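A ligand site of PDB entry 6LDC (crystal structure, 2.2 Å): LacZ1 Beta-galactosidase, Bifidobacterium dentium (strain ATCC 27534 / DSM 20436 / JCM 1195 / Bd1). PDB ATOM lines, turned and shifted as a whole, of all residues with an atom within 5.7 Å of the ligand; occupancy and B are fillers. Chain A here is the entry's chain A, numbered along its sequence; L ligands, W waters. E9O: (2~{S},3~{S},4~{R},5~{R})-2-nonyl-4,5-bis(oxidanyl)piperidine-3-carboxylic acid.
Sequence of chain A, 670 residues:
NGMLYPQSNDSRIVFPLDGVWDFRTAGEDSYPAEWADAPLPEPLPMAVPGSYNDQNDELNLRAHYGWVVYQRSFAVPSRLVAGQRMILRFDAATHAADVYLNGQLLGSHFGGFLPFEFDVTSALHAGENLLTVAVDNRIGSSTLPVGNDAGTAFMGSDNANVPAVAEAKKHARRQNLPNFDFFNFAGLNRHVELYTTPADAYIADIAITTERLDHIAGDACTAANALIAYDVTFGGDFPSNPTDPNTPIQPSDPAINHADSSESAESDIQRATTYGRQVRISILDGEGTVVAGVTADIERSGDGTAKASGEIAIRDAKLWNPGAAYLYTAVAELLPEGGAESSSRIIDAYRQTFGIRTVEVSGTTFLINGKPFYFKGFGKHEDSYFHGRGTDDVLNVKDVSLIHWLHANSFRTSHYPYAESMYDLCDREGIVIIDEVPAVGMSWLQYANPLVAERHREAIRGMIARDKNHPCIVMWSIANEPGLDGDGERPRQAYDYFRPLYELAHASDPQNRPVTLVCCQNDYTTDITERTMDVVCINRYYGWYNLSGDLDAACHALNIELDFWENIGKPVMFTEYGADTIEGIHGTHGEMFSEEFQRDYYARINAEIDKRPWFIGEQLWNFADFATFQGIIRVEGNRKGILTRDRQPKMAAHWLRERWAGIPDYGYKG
NE1 of Trp 621 sits at hydrogen-bond distance from O4 of the ligand. The side-chain carboxylate (OE1) of Glu 481 lies within salt-bridge range of a nitrogen (N) of the ligand (2.9 Å). O4 of the ligand sits at hydrogen-bond distance from OD2 of Asp 181, at 2.4 Å. The side-chain hydroxyl of Tyr 545 is in hydrogen-bond range of an oxygen (O62) of the ligand (2.7 Å). The guanidinium group (NH2) of Arg 634 lies within salt-bridge range of an oxygen (O62) of the ligand (3.0 Å). The side-chain amino group (NZ) of Lys 640 lies within salt-bridge range of an oxygen (O61) of the ligand. O61 of the ligand is in hydrogen-bond range of ND2 of Asn 638, 2.9 Å away. OE1 of Glu 576 is in salt-bridge range of N of the ligand, 2.8 Å away. O3 of the ligand is in hydrogen-bond range of NE2 of His 415 (2.7 Å).
The guanidinium group of Arg 634 is in hydrogen-bond range of the side-chain hydroxyl of Tyr 545, at 3.2 Å. NH1 of Arg 634 lies within salt-bridge range of OD2 of Asp 580 (3.6 Å). OD1 of Asn 480 lies within hydrogen-bond range of ND2 of Asn 539 (3.4 Å). ND2 of Asn 539 lies within hydrogen-bond range of OE2 of Glu 481 (3.0 Å). OH of Tyr 541 sits at hydrogen-bond distance from OE1 of Glu 576 (2.6 Å). The backbone NH (N) of Asn 638 lies within hydrogen-bond range of the backbone carbonyl oxygen (O) of Phe 626 (2.9 Å). N of Gln 521 is in hydrogen-bond range of O of Asn 539 (3.4 Å). The side-chain carboxylate (OD1) of Asp 181 is in salt-bridge range of the guanidinium group (NE) of Arg 634 (2.9 Å).
An oxygen (O62) of the ligand lies close to the side-chain sulfur (SD) of Met 155 (3.6 Å). Merely in contact with the ligand: Asn 480, Gln 521, Tyr 541, Asn 546 and Phe 626. Hydrophobic or aromatic side chains within 4 Å of the ligand: Met 155, His 415, Tyr 541, Tyr 545, Trp 621 and Phe 626. Of the 21 residues printed, 15 come within 4 Å of the ligand. The nearest printed residue that does not touch the ligand is Cys 520 (4.2 Å).
Water W3 lies within hydrogen-bond range of O3 of the ligand (2.6 Å), O of Asp 181 (2.7 Å) and NE2 of His 381 (2.8 Å). Water W2 lies within hydrogen-bond range of O3 of the ligand (2.8 Å) and N of Asp 181 (2.8 Å). Water W1 lies within hydrogen-bond range of OE2 of Glu 481, N of Gln 521 and O of Asn 539.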
ATOM      1  N   MET A 155     -12.594  -8.949   5.481  1.00  0.00           N
ATOM      2  CA  MET A 155     -13.504  -8.752   6.611  1.00  0.00           C
ATOM      3  C   MET A 155     -13.277  -7.377   7.228  1.00  0.00           C
ATOM      4  O   MET A 155     -13.006  -7.255   8.424  1.00  0.00           O
ATOM      5  CB  MET A 155     -13.308  -9.871   7.633  1.00  0.00           C
ATOM      6  CG  MET A 155     -13.578 -11.253   7.049  1.00  0.00           C
ATOM      7  SD  MET A 155     -13.353 -12.639   8.190  1.00  0.00           S
ATOM      8  CE  MET A 155     -11.715 -13.220   7.738  1.00  0.00           C
ATOM      9  N   ASP A 181      -6.768 -13.403   6.034  1.00  0.00           N
ATOM     10  CA  ASP A 181      -6.822 -13.116   7.463  1.00  0.00           C
ATOM     11  C   ASP A 181      -5.567 -13.545   8.196  1.00  0.00           C
ATOM     12  O   ASP A 181      -5.635 -14.312   9.158  1.00  0.00           O
ATOM     13  CB  ASP A 181      -8.049 -13.808   8.089  1.00  0.00           C
ATOM     14  CG  ASP A 181      -8.170 -13.566   9.590  1.00  0.00           C
ATOM     15  OD1 ASP A 181      -7.885 -12.459  10.066  1.00  0.00           O
ATOM     16  OD2 ASP A 181      -8.532 -14.519  10.312  1.00  0.00           O
ATOM     17  N   PHE A 182      -4.407 -13.107   7.711  1.00  0.00           N
ATOM     18  CA  PHE A 182      -3.166 -13.248   8.458  1.00  0.00           C
ATOM     19  C   PHE A 182      -2.205 -12.156   8.029  1.00  0.00           C
ATOM     20  O   PHE A 182      -2.239 -11.720   6.863  1.00  0.00           O
ATOM     21  CB  PHE A 182      -2.546 -14.651   8.309  1.00  0.00           C
ATOM     22  CG  PHE A 182      -2.245 -15.066   6.877  1.00  0.00           C
ATOM     23  CD1 PHE A 182      -0.979 -14.850   6.330  1.00  0.00           C
ATOM     24  CD2 PHE A 182      -3.195 -15.723   6.113  1.00  0.00           C
ATOM     25  CE1 PHE A 182      -0.670 -15.251   5.043  1.00  0.00           C
ATOM     26  CE2 PHE A 182      -2.896 -16.150   4.807  1.00  0.00           C
ATOM     27  CZ  PHE A 182      -1.626 -15.913   4.273  1.00  0.00           C
ATOM     28  N   HIS A 381      -0.638 -21.900  11.783  1.00  0.00           N
ATOM     29  CA  HIS A 381       0.084 -20.859  11.051  1.00  0.00           C
ATOM     30  C   HIS A 381       1.541 -20.943  11.465  1.00  0.00           C
ATOM     31  O   HIS A 381       1.852 -21.357  12.576  1.00  0.00           O
ATOM     32  CB  HIS A 381      -0.477 -19.456  11.352  1.00  0.00           C
ATOM     33  CG  HIS A 381      -1.428 -18.938  10.319  1.00  0.00           C
ATOM     34  ND1 HIS A 381      -1.055 -18.701   9.013  1.00  0.00           N
ATOM     35  CD2 HIS A 381      -2.743 -18.619  10.390  1.00  0.00           C
ATOM     36  CE1 HIS A 381      -2.106 -18.265   8.327  1.00  0.00           C
ATOM     37  NE2 HIS A 381      -3.137 -18.197   9.144  1.00  0.00           N
ATOM     38  N   HIS A 415      -1.766 -21.118   5.403  1.00  0.00           N
ATOM     39  CA  HIS A 415      -2.327 -21.234   4.054  1.00  0.00           C
ATOM     40  C   HIS A 415      -1.191 -21.090   3.027  1.00  0.00           C
ATOM     41  O   HIS A 415      -1.243 -20.211   2.164  1.00  0.00           O
ATOM     42  CB  HIS A 415      -3.379 -20.153   3.787  1.00  0.00           C
ATOM     43  CG  HIS A 415      -4.559 -20.214   4.711  1.00  0.00           C
ATOM     44  ND1 HIS A 415      -5.446 -21.280   4.733  1.00  0.00           N
ATOM     45  CD2 HIS A 415      -5.037 -19.310   5.605  1.00  0.00           C
ATOM     46  CE1 HIS A 415      -6.391 -21.036   5.616  1.00  0.00           C
ATOM     47  NE2 HIS A 415      -6.170 -19.845   6.157  1.00  0.00           N
ATOM     48  N   VAL A 440      -4.906 -18.416  -1.511  1.00  0.00           N
ATOM     49  CA  VAL A 440      -5.962 -17.954  -0.607  1.00  0.00           C
ATOM     50  C   VAL A 440      -6.347 -16.523  -1.000  1.00  0.00           C
ATOM     51  O   VAL A 440      -5.482 -15.715  -1.366  1.00  0.00           O
ATOM     52  CB  VAL A 440      -5.486 -18.024   0.878  1.00  0.00           C
ATOM     53  CG1 VAL A 440      -4.152 -17.265   1.055  1.00  0.00           C
ATOM     54  CG2 VAL A 440      -6.552 -17.507   1.829  1.00  0.00           C
ATOM     55  N   ASN A 480      -7.487 -22.272  -0.511  1.00  0.00           N
ATOM     56  CA  ASN A 480      -8.318 -22.040   0.658  1.00  0.00           C
ATOM     57  C   ASN A 480      -9.376 -20.973   0.425  1.00  0.00           C
ATOM     58  O   ASN A 480      -9.064 -19.819   0.101  1.00  0.00           O
ATOM     59  CB  ASN A 480      -7.480 -21.639   1.873  1.00  0.00           C
ATOM     60  CG  ASN A 480      -8.324 -21.382   3.100  1.00  0.00           C
ATOM     61  OD1 ASN A 480      -8.716 -22.323   3.810  1.00  0.00           O
ATOM     62  ND2 ASN A 480      -8.628 -20.109   3.358  1.00  0.00           N
ATOM     63  N   GLU A 481     -10.632 -21.367   0.597  1.00  0.00           N
ATOM     64  CA  GLU A 481     -11.795 -20.483   0.454  1.00  0.00           C
ATOM     65  C   GLU A 481     -11.833 -19.607  -0.814  1.00  0.00           C
ATOM     66  O   GLU A 481     -12.009 -18.393  -0.722  1.00  0.00           O
ATOM     67  CB  GLU A 481     -11.890 -19.586   1.699  1.00  0.00           C
ATOM     68  CG  GLU A 481     -12.041 -20.404   2.980  1.00  0.00           C
ATOM     69  CD  GLU A 481     -12.237 -19.542   4.210  1.00  0.00           C
ATOM     70  OE1 GLU A 481     -11.734 -18.402   4.226  1.00  0.00           O
ATOM     71  OE2 GLU A 481     -12.878 -20.015   5.177  1.00  0.00           O
ATOM     72  N   CYS A 520     -14.949 -22.400   1.453  1.00  0.00           N
ATOM     73  CA  CYS A 520     -15.541 -21.334   2.251  1.00  0.00           C
ATOM     74  C   CYS A 520     -16.984 -21.707   2.597  1.00  0.00           C
ATOM     75  O   CYS A 520     -17.623 -22.505   1.889  1.00  0.00           O
ATOM     76  CB  CYS A 520     -15.510 -20.011   1.474  1.00  0.00           C
ATOM     77  SG  CYS A 520     -15.853 -18.541   2.447  1.00  0.00           S
ATOM     78  N   GLN A 521     -17.476 -21.141   3.693  1.00  0.00           N
ATOM     79  CA  GLN A 521     -18.883 -21.232   4.038  1.00  0.00           C
ATOM     80  C   GLN A 521     -19.694 -20.494   2.981  1.00  0.00           C
ATOM     81  O   GLN A 521     -19.790 -19.270   3.018  1.00  0.00           O
ATOM     82  CB  GLN A 521     -19.136 -20.652   5.436  1.00  0.00           C
ATOM     83  CG  GLN A 521     -20.611 -20.590   5.842  1.00  0.00           C
ATOM     84  CD  GLN A 521     -20.796 -20.635   7.343  1.00  0.00           C
ATOM     85  OE1 GLN A 521     -19.824 -20.656   8.104  1.00  0.00           O
ATOM     86  NE2 GLN A 521     -22.045 -20.609   7.777  1.00  0.00           N
ATOM     87  N   ASN A 539     -14.996 -25.340   5.652  1.00  0.00           N
ATOM     88  CA  ASN A 539     -14.819 -24.352   6.711  1.00  0.00           C
ATOM     89  C   ASN A 539     -16.186 -23.807   7.112  1.00  0.00           C
ATOM     90  O   ASN A 539     -16.842 -23.155   6.294  1.00  0.00           O
ATOM     91  CB  ASN A 539     -13.908 -23.209   6.259  1.00  0.00           C
ATOM     92  CG  ASN A 539     -12.495 -23.655   5.978  1.00  0.00           C
ATOM     93  OD1 ASN A 539     -12.126 -24.801   6.224  1.00  0.00           O
ATOM     94  ND2 ASN A 539     -11.678 -22.731   5.470  1.00  0.00           N
ATOM     95  N   TYR A 541     -18.671 -21.855  10.178  1.00  0.00           N
ATOM     96  CA  TYR A 541     -18.698 -21.020  11.372  1.00  0.00           C
ATOM     97  C   TYR A 541     -20.123 -20.712  11.792  1.00  0.00           C
ATOM     98  O   TYR A 541     -20.423 -19.609  12.247  1.00  0.00           O
ATOM     99  CB  TYR A 541     -17.899 -19.743  11.123  1.00  0.00           C
ATOM    100  CG  TYR A 541     -16.404 -19.963  11.019  1.00  0.00           C
ATOM    101  CD1 TYR A 541     -15.818 -20.317   9.805  1.00  0.00           C
ATOM    102  CD2 TYR A 541     -15.586 -19.840  12.133  1.00  0.00           C
ATOM    103  CE1 TYR A 541     -14.454 -20.524   9.710  1.00  0.00           C
ATOM    104  CE2 TYR A 541     -14.216 -20.042  12.044  1.00  0.00           C
ATOM    105  CZ  TYR A 541     -13.662 -20.376  10.829  1.00  0.00           C
ATOM    106  OH  TYR A 541     -12.307 -20.573  10.751  1.00  0.00           O
ATOM    107  N   TYR A 545     -20.025 -16.590  12.880  1.00  0.00           N
ATOM    108  CA  TYR A 545     -20.253 -15.551  11.873  1.00  0.00           C
ATOM    109  C   TYR A 545     -21.715 -15.435  11.436  1.00  0.00           C
ATOM    110  O   TYR A 545     -22.103 -14.455  10.804  1.00  0.00           O
ATOM    111  CB  TYR A 545     -19.357 -15.776  10.648  1.00  0.00           C
ATOM    112  CG  TYR A 545     -17.903 -15.409  10.886  1.00  0.00           C
ATOM    113  CD1 TYR A 545     -17.547 -14.148  11.364  1.00  0.00           C
ATOM    114  CD2 TYR A 545     -16.892 -16.339  10.665  1.00  0.00           C
ATOM    115  CE1 TYR A 545     -16.203 -13.805  11.586  1.00  0.00           C
ATOM    116  CE2 TYR A 545     -15.554 -16.010  10.887  1.00  0.00           C
ATOM    117  CZ  TYR A 545     -15.212 -14.749  11.347  1.00  0.00           C
ATOM    118  OH  TYR A 545     -13.890 -14.451  11.561  1.00  0.00           O
ATOM    119  N   ASN A 546     -22.524 -16.459  11.722  1.00  0.00           N
ATOM    120  CA  ASN A 546     -23.967 -16.330  11.552  1.00  0.00           C
ATOM    121  C   ASN A 546     -24.653 -17.075  12.682  1.00  0.00           C
ATOM    122  O   ASN A 546     -23.973 -17.815  13.400  1.00  0.00           O
ATOM    123  CB  ASN A 546     -24.452 -16.865  10.198  1.00  0.00           C
ATOM    124  CG  ASN A 546     -24.057 -18.318   9.943  1.00  0.00           C
ATOM    125  OD1 ASN A 546     -24.049 -19.151  10.847  1.00  0.00           O
ATOM    126  ND2 ASN A 546     -23.777 -18.626   8.693  1.00  0.00           N
ATOM    127  N   GLU A 576     -11.863 -26.064   9.109  1.00  0.00           N
ATOM    128  CA  GLU A 576     -11.972 -24.895  10.004  1.00  0.00           C
ATOM    129  C   GLU A 576     -13.324 -24.855  10.696  1.00  0.00           C
ATOM    130  O   GLU A 576     -14.350 -25.177  10.084  1.00  0.00           O
ATOM    131  CB  GLU A 576     -11.802 -23.561   9.254  1.00  0.00           C
ATOM    132  CG  GLU A 576     -10.419 -23.306   8.689  1.00  0.00           C
ATOM    133  CD  GLU A 576     -10.288 -21.932   8.095  1.00  0.00           C
ATOM    134  OE1 GLU A 576     -11.110 -21.045   8.453  1.00  0.00           O
ATOM    135  OE2 GLU A 576      -9.387 -21.741   7.237  1.00  0.00           O
ATOM    136  N   ASP A 580     -13.614 -16.744  18.268  1.00  0.00           N
ATOM    137  CA  ASP A 580     -12.600 -15.909  18.907  1.00  0.00           C
ATOM    138  C   ASP A 580     -12.807 -15.952  20.397  1.00  0.00           C
ATOM    139  O   ASP A 580     -13.948 -15.896  20.892  1.00  0.00           O
ATOM    140  CB  ASP A 580     -12.652 -14.473  18.368  1.00  0.00           C
ATOM    141  CG  ASP A 580     -12.121 -14.363  16.954  1.00  0.00           C
ATOM    142  OD1 ASP A 580     -12.885 -14.690  16.014  1.00  0.00           O
ATOM    143  OD2 ASP A 580     -10.952 -13.957  16.780  1.00  0.00           O
ATOM    144  N   TRP A 621     -10.257 -24.399  13.669  1.00  0.00           N
ATOM    145  CA  TRP A 621      -9.489 -23.174  13.510  1.00  0.00           C
ATOM    146  C   TRP A 621      -9.504 -22.449  14.844  1.00  0.00           C
ATOM    147  O   TRP A 621     -10.594 -22.146  15.320  1.00  0.00           O
ATOM    148  CB  TRP A 621     -10.103 -22.306  12.411  1.00  0.00           C
ATOM    149  CG  TRP A 621      -9.258 -21.188  11.916  1.00  0.00           C
ATOM    150  CD1 TRP A 621      -9.436 -19.841  12.150  1.00  0.00           C
ATOM    151  CD2 TRP A 621      -8.112 -21.299  11.066  1.00  0.00           C
ATOM    152  NE1 TRP A 621      -8.463 -19.117  11.496  1.00  0.00           N
ATOM    153  CE2 TRP A 621      -7.633 -19.986  10.821  1.00  0.00           C
ATOM    154  CE3 TRP A 621      -7.433 -22.379  10.484  1.00  0.00           C
ATOM    155  CZ2 TRP A 621      -6.515 -19.732  10.034  1.00  0.00           C
ATOM    156  CZ3 TRP A 621      -6.322 -22.121   9.686  1.00  0.00           C
ATOM    157  CH2 TRP A 621      -5.886 -20.808   9.469  1.00  0.00           C
ATOM    158  N   PHE A 626      -3.007 -15.943  16.374  1.00  0.00           N
ATOM    159  CA  PHE A 626      -1.986 -15.484  15.441  1.00  0.00           C
ATOM    160  C   PHE A 626      -2.225 -14.053  14.966  1.00  0.00           C
ATOM    161  O   PHE A 626      -3.341 -13.541  15.089  1.00  0.00           O
ATOM    162  CB  PHE A 626      -1.890 -16.444  14.246  1.00  0.00           C
ATOM    163  CG  PHE A 626      -3.163 -16.553  13.438  1.00  0.00           C
ATOM    164  CD1 PHE A 626      -4.107 -17.540  13.732  1.00  0.00           C
ATOM    165  CD2 PHE A 626      -3.414 -15.686  12.378  1.00  0.00           C
ATOM    166  CE1 PHE A 626      -5.273 -17.663  12.973  1.00  0.00           C
ATOM    167  CE2 PHE A 626      -4.572 -15.812  11.613  1.00  0.00           C
ATOM    168  CZ  PHE A 626      -5.508 -16.802  11.919  1.00  0.00           C
ATOM    169  N   ARG A 634     -10.658  -7.973  15.067  1.00  0.00           N
ATOM    170  CA  ARG A 634      -9.408  -8.628  15.445  1.00  0.00           C
ATOM    171  C   ARG A 634      -8.762  -8.055  16.701  1.00  0.00           C
ATOM    172  O   ARG A 634      -8.098  -7.021  16.655  1.00  0.00           O
ATOM    173  CB  ARG A 634      -8.419  -8.572  14.261  1.00  0.00           C
ATOM    174  CG  ARG A 634      -8.847  -9.478  13.082  1.00  0.00           C
ATOM    175  CD  ARG A 634      -8.780 -10.936  13.476  1.00  0.00           C
ATOM    176  NE  ARG A 634      -9.375 -11.760  12.433  1.00  0.00           N
ATOM    177  CZ  ARG A 634     -10.583 -12.313  12.503  1.00  0.00           C
ATOM    178  NH1 ARG A 634     -11.322 -12.198  13.607  1.00  0.00           N
ATOM    179  NH2 ARG A 634     -11.014 -13.034  11.474  1.00  0.00           N
ATOM    180  N   ASN A 638      -6.080 -12.720  15.293  1.00  0.00           N
ATOM    181  CA  ASN A 638      -7.108 -13.753  15.317  1.00  0.00           C
ATOM    182  C   ASN A 638      -7.035 -14.538  16.623  1.00  0.00           C
ATOM    183  O   ASN A 638      -5.998 -15.099  16.964  1.00  0.00           O
ATOM    184  CB  ASN A 638      -6.945 -14.686  14.113  1.00  0.00           C
ATOM    185  CG  ASN A 638      -8.124 -15.620  13.934  1.00  0.00           C
ATOM    186  OD1 ASN A 638      -8.418 -16.432  14.802  1.00  0.00           O
ATOM    187  ND2 ASN A 638      -8.803 -15.508  12.786  1.00  0.00           N
ATOM    188  N   LYS A 640      -9.049 -17.184  17.551  1.00  0.00           N
ATOM    189  CA  LYS A 640      -9.712 -18.487  17.502  1.00  0.00           C
ATOM    190  C   LYS A 640      -8.789 -19.645  17.896  1.00  0.00           C
ATOM    191  O   LYS A 640      -9.194 -20.814  17.853  1.00  0.00           O
ATOM    192  CB  LYS A 640     -10.310 -18.731  16.114  1.00  0.00           C
ATOM    193  CG  LYS A 640     -11.416 -17.746  15.733  1.00  0.00           C
ATOM    194  CD  LYS A 640     -12.156 -18.168  14.467  1.00  0.00           C
ATOM    195  CE  LYS A 640     -13.217 -17.137  14.054  1.00  0.00           C
ATOM    196  NZ  LYS A 640     -12.615 -15.806  13.669  1.00  0.00           N
HETATM  197  C2  E9O L   1      -9.779 -18.526   6.670  1.00  0.00           C
HETATM  198  C3  E9O L   1      -8.812 -18.212   7.822  1.00  0.00           C
HETATM  199  O3  E9O L   1      -7.538 -17.854   7.269  1.00  0.00           O
HETATM  200  N   E9O L   1     -11.169 -18.560   7.115  1.00  0.00           N
HETATM  201  C7  E9O L   1     -11.632 -17.519   8.031  1.00  0.00           C
HETATM  202  C5  E9O L   1     -10.723 -17.504   9.253  1.00  0.00           C
HETATM  203  C6  E9O L   1     -11.223 -16.538  10.316  1.00  0.00           C
HETATM  204  O62 E9O L   1     -11.877 -15.429   9.980  1.00  0.00           O
HETATM  205  C4  E9O L   1      -9.357 -17.100   8.732  1.00  0.00           C
HETATM  206  O4  E9O L   1      -8.482 -16.877   9.839  1.00  0.00           O
HETATM  207  O61 E9O L   1     -11.041 -16.775  11.498  1.00  0.00           O
HETATM  208  C8  E9O L   1     -13.091 -17.741   8.370  1.00  0.00           C
HETATM  209  C9  E9O L   1     -13.916 -17.310   7.164  1.00  0.00           C
HETATM  210  C10 E9O L   1     -15.373 -17.494   7.487  1.00  0.00           C
HETATM  211  C1  E9O L   1     -16.256 -16.975   6.352  1.00  0.00           C
HETATM  212  C11 E9O L   1     -17.673 -17.461   6.614  1.00  0.00           C
HETATM  213  C12 E9O L   1     -18.677 -16.316   6.541  1.00  0.00           C
HETATM  214  C13 E9O L   1     -20.056 -16.846   6.931  1.00  0.00           C
HETATM  215  C14 E9O L   1     -21.150 -15.913   6.433  1.00  0.00           C
HETATM  216  C15 E9O L   1     -22.498 -16.384   6.923  1.00  0.00           C
HETATM  217  O   HOH W   1     -15.572 -20.364   5.812  1.00  0.00           O
HETATM  218  O   HOH W   2      -7.688 -15.959   5.268  1.00  0.00           O
HETATM  219  O   HOH W   3      -5.467 -16.889   8.444  1.00  0.00           O
